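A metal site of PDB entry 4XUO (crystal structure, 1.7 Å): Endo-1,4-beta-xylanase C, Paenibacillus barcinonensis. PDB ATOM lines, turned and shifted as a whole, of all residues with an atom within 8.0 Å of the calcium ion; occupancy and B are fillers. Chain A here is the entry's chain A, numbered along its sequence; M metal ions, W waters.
N of Ser 15 is in hydrogen-bond range of OE1 of Gln 22, 3.5 Å away. The side-chain amide oxygen (OE1) of Gln 44 lies close to the backbone carbonyl oxygen (O) of Phe 16 (3.0 Å). OE1 of Gln 44 sits close to O of Glu 18, 2.9 Å away. The side-chain carboxylate (OE1) of Glu 17 lies within hydrogen-bond range of the backbone NH (N) of Lys 43. The backbone NH of Tyr 40 lies close to the side-chain carboxylate of Asp 149.
The calcium ion is bound by water W1 (2.3 Å), O of Ser 15 (2.4 Å), O of Gln 44 (2.4 Å), OE2 of Glu 17 (2.4 Å), OD1 of Asp 149 (2.5 Å), O of Gln 41 (2.5 Å) and OD2 of Asp 149 (2.6 Å).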
ATOM      1  N   HIS A  14      17.291   1.595  20.525  1.00  0.00           N
ATOM      2  CA  HIS A  14      16.915   0.704  19.428  1.00  0.00           C
ATOM      3  C   HIS A  14      17.949  -0.372  19.158  1.00  0.00           C
ATOM      4  O   HIS A  14      19.076  -0.078  18.695  1.00  0.00           O
ATOM      5  CB  HIS A  14      16.721   1.496  18.144  1.00  0.00           C
ATOM      6  CG  HIS A  14      15.570   2.440  18.164  1.00  0.00           C
ATOM      7  ND1 HIS A  14      15.370   3.351  17.156  1.00  0.00           N
ATOM      8  CD2 HIS A  14      14.553   2.612  19.038  1.00  0.00           C
ATOM      9  CE1 HIS A  14      14.251   4.011  17.371  1.00  0.00           C
ATOM     10  NE2 HIS A  14      13.750   3.606  18.534  1.00  0.00           N
ATOM     11  N   SER A  15      17.560  -1.612  19.440  1.00  0.00           N
ATOM     12  CA  SER A  15      18.408  -2.803  19.199  1.00  0.00           C
ATOM     13  C   SER A  15      18.067  -3.572  17.919  1.00  0.00           C
ATOM     14  O   SER A  15      18.871  -4.404  17.451  1.00  0.00           O
ATOM     15  CB  SER A  15      18.287  -3.755  20.386  1.00  0.00           C
ATOM     16  OG  SER A  15      17.000  -4.329  20.397  1.00  0.00           O
ATOM     17  N   PHE A  16      16.864  -3.309  17.386  1.00  0.00           N
ATOM     18  CA  PHE A  16      16.379  -3.878  16.122  1.00  0.00           C
ATOM     19  C   PHE A  16      16.137  -5.396  16.189  1.00  0.00           C
ATOM     20  O   PHE A  16      15.985  -6.033  15.162  1.00  0.00           O
ATOM     21  CB  PHE A  16      17.291  -3.502  14.941  1.00  0.00           C
ATOM     22  CG  PHE A  16      17.416  -2.001  14.755  1.00  0.00           C
ATOM     23  CD1 PHE A  16      16.297  -1.267  14.415  1.00  0.00           C
ATOM     24  CD2 PHE A  16      18.603  -1.329  15.040  1.00  0.00           C
ATOM     25  CE1 PHE A  16      16.368   0.117  14.283  1.00  0.00           C
ATOM     26  CE2 PHE A  16      18.692   0.046  14.897  1.00  0.00           C
ATOM     27  CZ  PHE A  16      17.558   0.773  14.530  1.00  0.00           C
ATOM     28  N   GLU A  17      16.028  -5.908  17.408  1.00  0.00           N
ATOM     29  CA  GLU A  17      15.972  -7.338  17.677  1.00  0.00           C
ATOM     30  C   GLU A  17      14.580  -7.937  17.549  1.00  0.00           C
ATOM     31  O   GLU A  17      14.438  -9.164  17.541  1.00  0.00           O
ATOM     32  CB  GLU A  17      16.511  -7.609  19.070  1.00  0.00           C
ATOM     33  CG  GLU A  17      17.991  -7.314  19.215  1.00  0.00           C
ATOM     34  CD  GLU A  17      18.856  -8.102  18.270  1.00  0.00           C
ATOM     35  OE1 GLU A  17      18.750  -9.349  18.261  1.00  0.00           O
ATOM     36  OE2 GLU A  17      19.677  -7.506  17.545  1.00  0.00           O
ATOM     37  N   GLU A  18      13.551  -7.090  17.449  1.00  0.00           N
ATOM     38  CA  GLU A  18      12.204  -7.549  17.157  1.00  0.00           C
ATOM     39  C   GLU A  18      11.997  -7.445  15.636  1.00  0.00           C
ATOM     40  O   GLU A  18      12.964  -7.388  14.879  1.00  0.00           O
ATOM     41  CB  GLU A  18      11.179  -6.724  17.957  1.00  0.00           C
ATOM     42  CG  GLU A  18      11.139  -7.066  19.447  1.00  0.00           C
ATOM     43  CD  GLU A  18      12.287  -6.454  20.243  1.00  0.00           C
ATOM     44  OE1 GLU A  18      12.388  -5.212  20.300  1.00  0.00           O
ATOM     45  OE2 GLU A  18      13.081  -7.227  20.835  1.00  0.00           O
ATOM     46  N   GLN A  22      11.257   0.206  14.226  1.00  0.00           N
ATOM     47  CA  GLN A  22      11.158   0.994  15.435  1.00  0.00           C
ATOM     48  C   GLN A  22      11.056   2.501  15.106  1.00  0.00           C
ATOM     49  O   GLN A  22      11.578   3.323  15.836  1.00  0.00           O
ATOM     50  CB  GLN A  22      12.331   0.713  16.384  1.00  0.00           C
ATOM     51  CG  GLN A  22      12.527  -0.765  16.717  1.00  0.00           C
ATOM     52  CD  GLN A  22      13.441  -0.984  17.924  1.00  0.00           C
ATOM     53  OE1 GLN A  22      14.518  -1.564  17.802  1.00  0.00           O
ATOM     54  NE2 GLN A  22      13.035  -0.492  19.074  1.00  0.00           N
ATOM     55  N   VAL A  34      14.926  -4.310   8.571  1.00  0.00           N
ATOM     56  CA  VAL A  34      15.778  -5.060   9.496  1.00  0.00           C
ATOM     57  C   VAL A  34      16.405  -6.268   8.788  1.00  0.00           C
ATOM     58  O   VAL A  34      15.783  -6.890   7.895  1.00  0.00           O
ATOM     59  CB  VAL A  34      14.979  -5.435  10.750  1.00  0.00           C
ATOM     60  CG1 VAL A  34      15.820  -6.250  11.709  1.00  0.00           C
ATOM     61  CG2 VAL A  34      14.492  -4.164  11.427  1.00  0.00           C
ATOM     62  N   THR A  35      17.665  -6.570   9.139  1.00  0.00           N
ATOM     63  CA  THR A  35      18.366  -7.714   8.581  1.00  0.00           C
ATOM     64  C   THR A  35      18.920  -8.577   9.697  1.00  0.00           C
ATOM     65  O   THR A  35      19.374  -8.062  10.727  1.00  0.00           O
ATOM     66  CB  THR A  35      19.550  -7.307   7.661  1.00  0.00           C
ATOM     67  OG1 THR A  35      20.147  -8.479   7.081  1.00  0.00           O
ATOM     68  CG2 THR A  35      20.635  -6.538   8.407  1.00  0.00           C
ATOM     69  N   GLN A  38      23.702  -9.332   9.502  1.00  0.00           N
ATOM     70  CA  GLN A  38      24.802  -8.638  10.206  1.00  0.00           C
ATOM     71  C   GLN A  38      24.238  -7.953  11.428  1.00  0.00           C
ATOM     72  O   GLN A  38      23.089  -7.527  11.411  1.00  0.00           O
ATOM     73  CB  GLN A  38      25.389  -7.558   9.303  1.00  0.00           C
ATOM     74  CG  GLN A  38      26.073  -8.027   8.034  1.00  0.00           C
ATOM     75  CD  GLN A  38      27.487  -8.488   8.274  1.00  0.00           C
ATOM     76  OE1 GLN A  38      28.169  -8.007   9.173  1.00  0.00           O
ATOM     77  NE2 GLN A  38      27.943  -9.422   7.466  1.00  0.00           N
ATOM     78  N   ALA A  39      25.056  -7.802  12.477  1.00  0.00           N
ATOM     79  CA  ALA A  39      24.638  -7.063  13.674  1.00  0.00           C
ATOM     80  C   ALA A  39      25.846  -6.708  14.521  1.00  0.00           C
ATOM     81  O   ALA A  39      26.875  -7.386  14.465  1.00  0.00           O
ATOM     82  CB  ALA A  39      23.628  -7.851  14.492  1.00  0.00           C
ATOM     83  N   TYR A  40      25.720  -5.641  15.309  1.00  0.00           N
ATOM     84  CA  TYR A  40      26.796  -5.259  16.192  1.00  0.00           C
ATOM     85  C   TYR A  40      26.560  -5.919  17.553  1.00  0.00           C
ATOM     86  O   TYR A  40      27.520  -6.354  18.189  1.00  0.00           O
ATOM     87  CB  TYR A  40      26.927  -3.733  16.311  1.00  0.00           C
ATOM     88  CG  TYR A  40      27.851  -3.318  17.432  1.00  0.00           C
ATOM     89  CD1 TYR A  40      29.234  -3.382  17.277  1.00  0.00           C
ATOM     90  CD2 TYR A  40      27.338  -2.914  18.648  1.00  0.00           C
ATOM     91  CE1 TYR A  40      30.078  -3.020  18.334  1.00  0.00           C
ATOM     92  CE2 TYR A  40      28.171  -2.561  19.688  1.00  0.00           C
ATOM     93  CZ  TYR A  40      29.536  -2.613  19.522  1.00  0.00           C
ATOM     94  OH  TYR A  40      30.323  -2.254  20.602  1.00  0.00           O
ATOM     95  N   GLN A  41      25.292  -5.956  17.967  1.00  0.00           N
ATOM     96  CA  GLN A  41      24.808  -6.654  19.145  1.00  0.00           C
ATOM     97  C   GLN A  41      23.562  -7.468  18.786  1.00  0.00           C
ATOM     98  O   GLN A  41      22.752  -7.050  17.951  1.00  0.00           O
ATOM     99  CB  GLN A  41      24.414  -5.660  20.216  1.00  0.00           C
ATOM    100  CG  GLN A  41      24.462  -6.213  21.617  1.00  0.00           C
ATOM    101  CD  GLN A  41      25.886  -6.283  22.131  1.00  0.00           C
ATOM    102  OE1 GLN A  41      26.774  -5.574  21.649  1.00  0.00           O
ATOM    103  NE2 GLN A  41      26.112  -7.123  23.132  1.00  0.00           N
ATOM    104  N   GLY A  42      23.386  -8.629  19.430  1.00  0.00           N
ATOM    105  CA  GLY A  42      22.234  -9.470  19.128  1.00  0.00           C
ATOM    106  C   GLY A  42      22.307 -10.053  17.723  1.00  0.00           C
ATOM    107  O   GLY A  42      23.398 -10.315  17.194  1.00  0.00           O
ATOM    108  N   LYS A  43      21.153 -10.275  17.117  1.00  0.00           N
ATOM    109  CA  LYS A  43      21.106 -10.963  15.832  1.00  0.00           C
ATOM    110  C   LYS A  43      20.807 -10.044  14.661  1.00  0.00           C
ATOM    111  O   LYS A  43      21.048 -10.416  13.520  1.00  0.00           O
ATOM    112  CB  LYS A  43      20.041 -12.083  15.857  1.00  0.00           C
ATOM    113  CG  LYS A  43      20.084 -12.980  17.091  1.00  0.00           C
ATOM    114  CD  LYS A  43      19.156 -14.193  16.964  1.00  0.00           C
ATOM    115  CE  LYS A  43      17.692 -13.822  17.156  1.00  0.00           C
ATOM    116  NZ  LYS A  43      16.787 -14.984  16.937  1.00  0.00           N
ATOM    117  N   GLN A  44      20.299  -8.838  14.944  1.00  0.00           N
ATOM    118  CA  GLN A  44      19.728  -8.002  13.894  1.00  0.00           C
ATOM    119  C   GLN A  44      20.198  -6.567  13.926  1.00  0.00           C
ATOM    120  O   GLN A  44      20.591  -6.063  14.968  1.00  0.00           O
ATOM    121  CB  GLN A  44      18.202  -8.034  13.995  1.00  0.00           C
ATOM    122  CG  GLN A  44      17.632  -9.405  13.666  1.00  0.00           C
ATOM    123  CD  GLN A  44      16.116  -9.398  13.613  1.00  0.00           C
ATOM    124  OE1 GLN A  44      15.443  -8.907  14.514  1.00  0.00           O
ATOM    125  NE2 GLN A  44      15.581  -9.927  12.525  1.00  0.00           N
ATOM    126  N   SER A  45      20.145  -5.920  12.763  1.00  0.00           N
ATOM    127  CA  SER A  45      20.464  -4.497  12.639  1.00  0.00           C
ATOM    128  C   SER A  45      19.576  -3.862  11.582  1.00  0.00           C
ATOM    129  O   SER A  45      18.836  -4.577  10.891  1.00  0.00           O
ATOM    130  CB  SER A  45      21.965  -4.297  12.301  1.00  0.00           C
ATOM    131  OG  SER A  45      22.294  -4.835  11.016  1.00  0.00           O
ATOM    132  N   LEU A  46      19.656  -2.537  11.438  1.00  0.00           N
ATOM    133  CA  LEU A  46      18.845  -1.800  10.464  1.00  0.00           C
ATOM    134  C   LEU A  46      19.639  -1.553   9.186  1.00  0.00           C
ATOM    135  O   LEU A  46      20.723  -0.945   9.232  1.00  0.00           O
ATOM    136  CB  LEU A  46      18.429  -0.424  11.016  1.00  0.00           C
ATOM    137  CG  LEU A  46      17.448   0.344  10.113  1.00  0.00           C
ATOM    138  CD1 LEU A  46      16.040  -0.236  10.173  1.00  0.00           C
ATOM    139  CD2 LEU A  46      17.431   1.819  10.505  1.00  0.00           C
ATOM    140  N   TRP A 118      32.537  -2.591  12.573  1.00  0.00           N
ATOM    141  CA  TRP A 118      31.587  -1.613  13.087  1.00  0.00           C
ATOM    142  C   TRP A 118      32.300  -0.402  13.674  1.00  0.00           C
ATOM    143  O   TRP A 118      33.366  -0.546  14.303  1.00  0.00           O
ATOM    144  CB  TRP A 118      30.676  -2.248  14.144  1.00  0.00           C
ATOM    145  CG  TRP A 118      29.793  -3.290  13.585  1.00  0.00           C
ATOM    146  CD1 TRP A 118      30.074  -4.636  13.471  1.00  0.00           C
ATOM    147  CD2 TRP A 118      28.464  -3.111  13.084  1.00  0.00           C
ATOM    148  NE1 TRP A 118      29.002  -5.294  12.894  1.00  0.00           N
ATOM    149  CE2 TRP A 118      28.001  -4.381  12.655  1.00  0.00           C
ATOM    150  CE3 TRP A 118      27.623  -2.010  12.958  1.00  0.00           C
ATOM    151  CZ2 TRP A 118      26.742  -4.567  12.094  1.00  0.00           C
ATOM    152  CZ3 TRP A 118      26.352  -2.188  12.416  1.00  0.00           C
ATOM    153  CH2 TRP A 118      25.926  -3.458  11.989  1.00  0.00           C
ATOM    154  N   LEU A 148      22.981   0.098  10.661  1.00  0.00           N
ATOM    155  CA  LEU A 148      22.966   0.774  11.959  1.00  0.00           C
ATOM    156  C   LEU A 148      22.496  -0.167  13.054  1.00  0.00           C
ATOM    157  O   LEU A 148      21.470  -0.871  12.879  1.00  0.00           O
ATOM    158  CB  LEU A 148      22.017   1.999  11.900  1.00  0.00           C
ATOM    159  CG  LEU A 148      21.755   2.756  13.205  1.00  0.00           C
ATOM    160  CD1 LEU A 148      23.009   3.453  13.699  1.00  0.00           C
ATOM    161  CD2 LEU A 148      20.611   3.756  13.087  1.00  0.00           C
ATOM    162  N   ASP A 149      23.165  -0.146  14.190  1.00  0.00           N
ATOM    163  CA  ASP A 149      22.712  -0.963  15.347  1.00  0.00           C
ATOM    164  C   ASP A 149      22.987  -0.251  16.685  1.00  0.00           C
ATOM    165  O   ASP A 149      23.778   0.687  16.747  1.00  0.00           O
ATOM    166  CB  ASP A 149      23.399  -2.340  15.323  1.00  0.00           C
ATOM    167  CG  ASP A 149      22.616  -3.422  16.075  1.00  0.00           C
ATOM    168  OD1 ASP A 149      21.450  -3.165  16.555  1.00  0.00           O
ATOM    169  OD2 ASP A 149      23.158  -4.551  16.168  1.00  0.00           O
ATOM    170  N   GLU A 150      22.340  -0.706  17.755  1.00  0.00           N
ATOM    171  CA  GLU A 150      22.541  -0.167  19.106  1.00  0.00           C
ATOM    172  C   GLU A 150      22.454   1.357  19.075  1.00  0.00           C
ATOM    173  O   GLU A 150      23.354   2.050  19.525  1.00  0.00           O
ATOM    174  CB  GLU A 150      23.852  -0.662  19.734  1.00  0.00           C
ATOM    175  CG  GLU A 150      23.779  -2.113  20.187  1.00  0.00           C
ATOM    176  CD  GLU A 150      22.800  -2.335  21.333  1.00  0.00           C
ATOM    177  OE1 GLU A 150      23.196  -2.127  22.504  1.00  0.00           O
ATOM    178  OE2 GLU A 150      21.638  -2.717  21.067  1.00  0.00           O
ATOM    179  N   PHE A 151      21.368   1.845  18.510  1.00  0.00           N
ATOM    180  CA  PHE A 151      21.109   3.290  18.457  1.00  0.00           C
ATOM    181  C   PHE A 151      20.528   3.762  19.782  1.00  0.00           C
ATOM    182  O   PHE A 151      19.712   3.059  20.386  1.00  0.00           O
ATOM    183  CB  PHE A 151      20.166   3.616  17.293  1.00  0.00           C
ATOM    184  CG  PHE A 151      19.797   5.074  17.214  1.00  0.00           C
ATOM    185  CD1 PHE A 151      20.656   6.012  16.670  1.00  0.00           C
ATOM    186  CD2 PHE A 151      18.560   5.495  17.674  1.00  0.00           C
ATOM    187  CE1 PHE A 151      20.308   7.347  16.612  1.00  0.00           C
ATOM    188  CE2 PHE A 151      18.195   6.829  17.626  1.00  0.00           C
ATOM    189  CZ  PHE A 151      19.068   7.767  17.085  1.00  0.00           C
HETATM  190 CA    CA M   1      20.987  -5.479  17.252  1.00  0.00          CA
HETATM  191  O   HOH W   1      21.304  -4.932  19.498  1.00  0.00           O
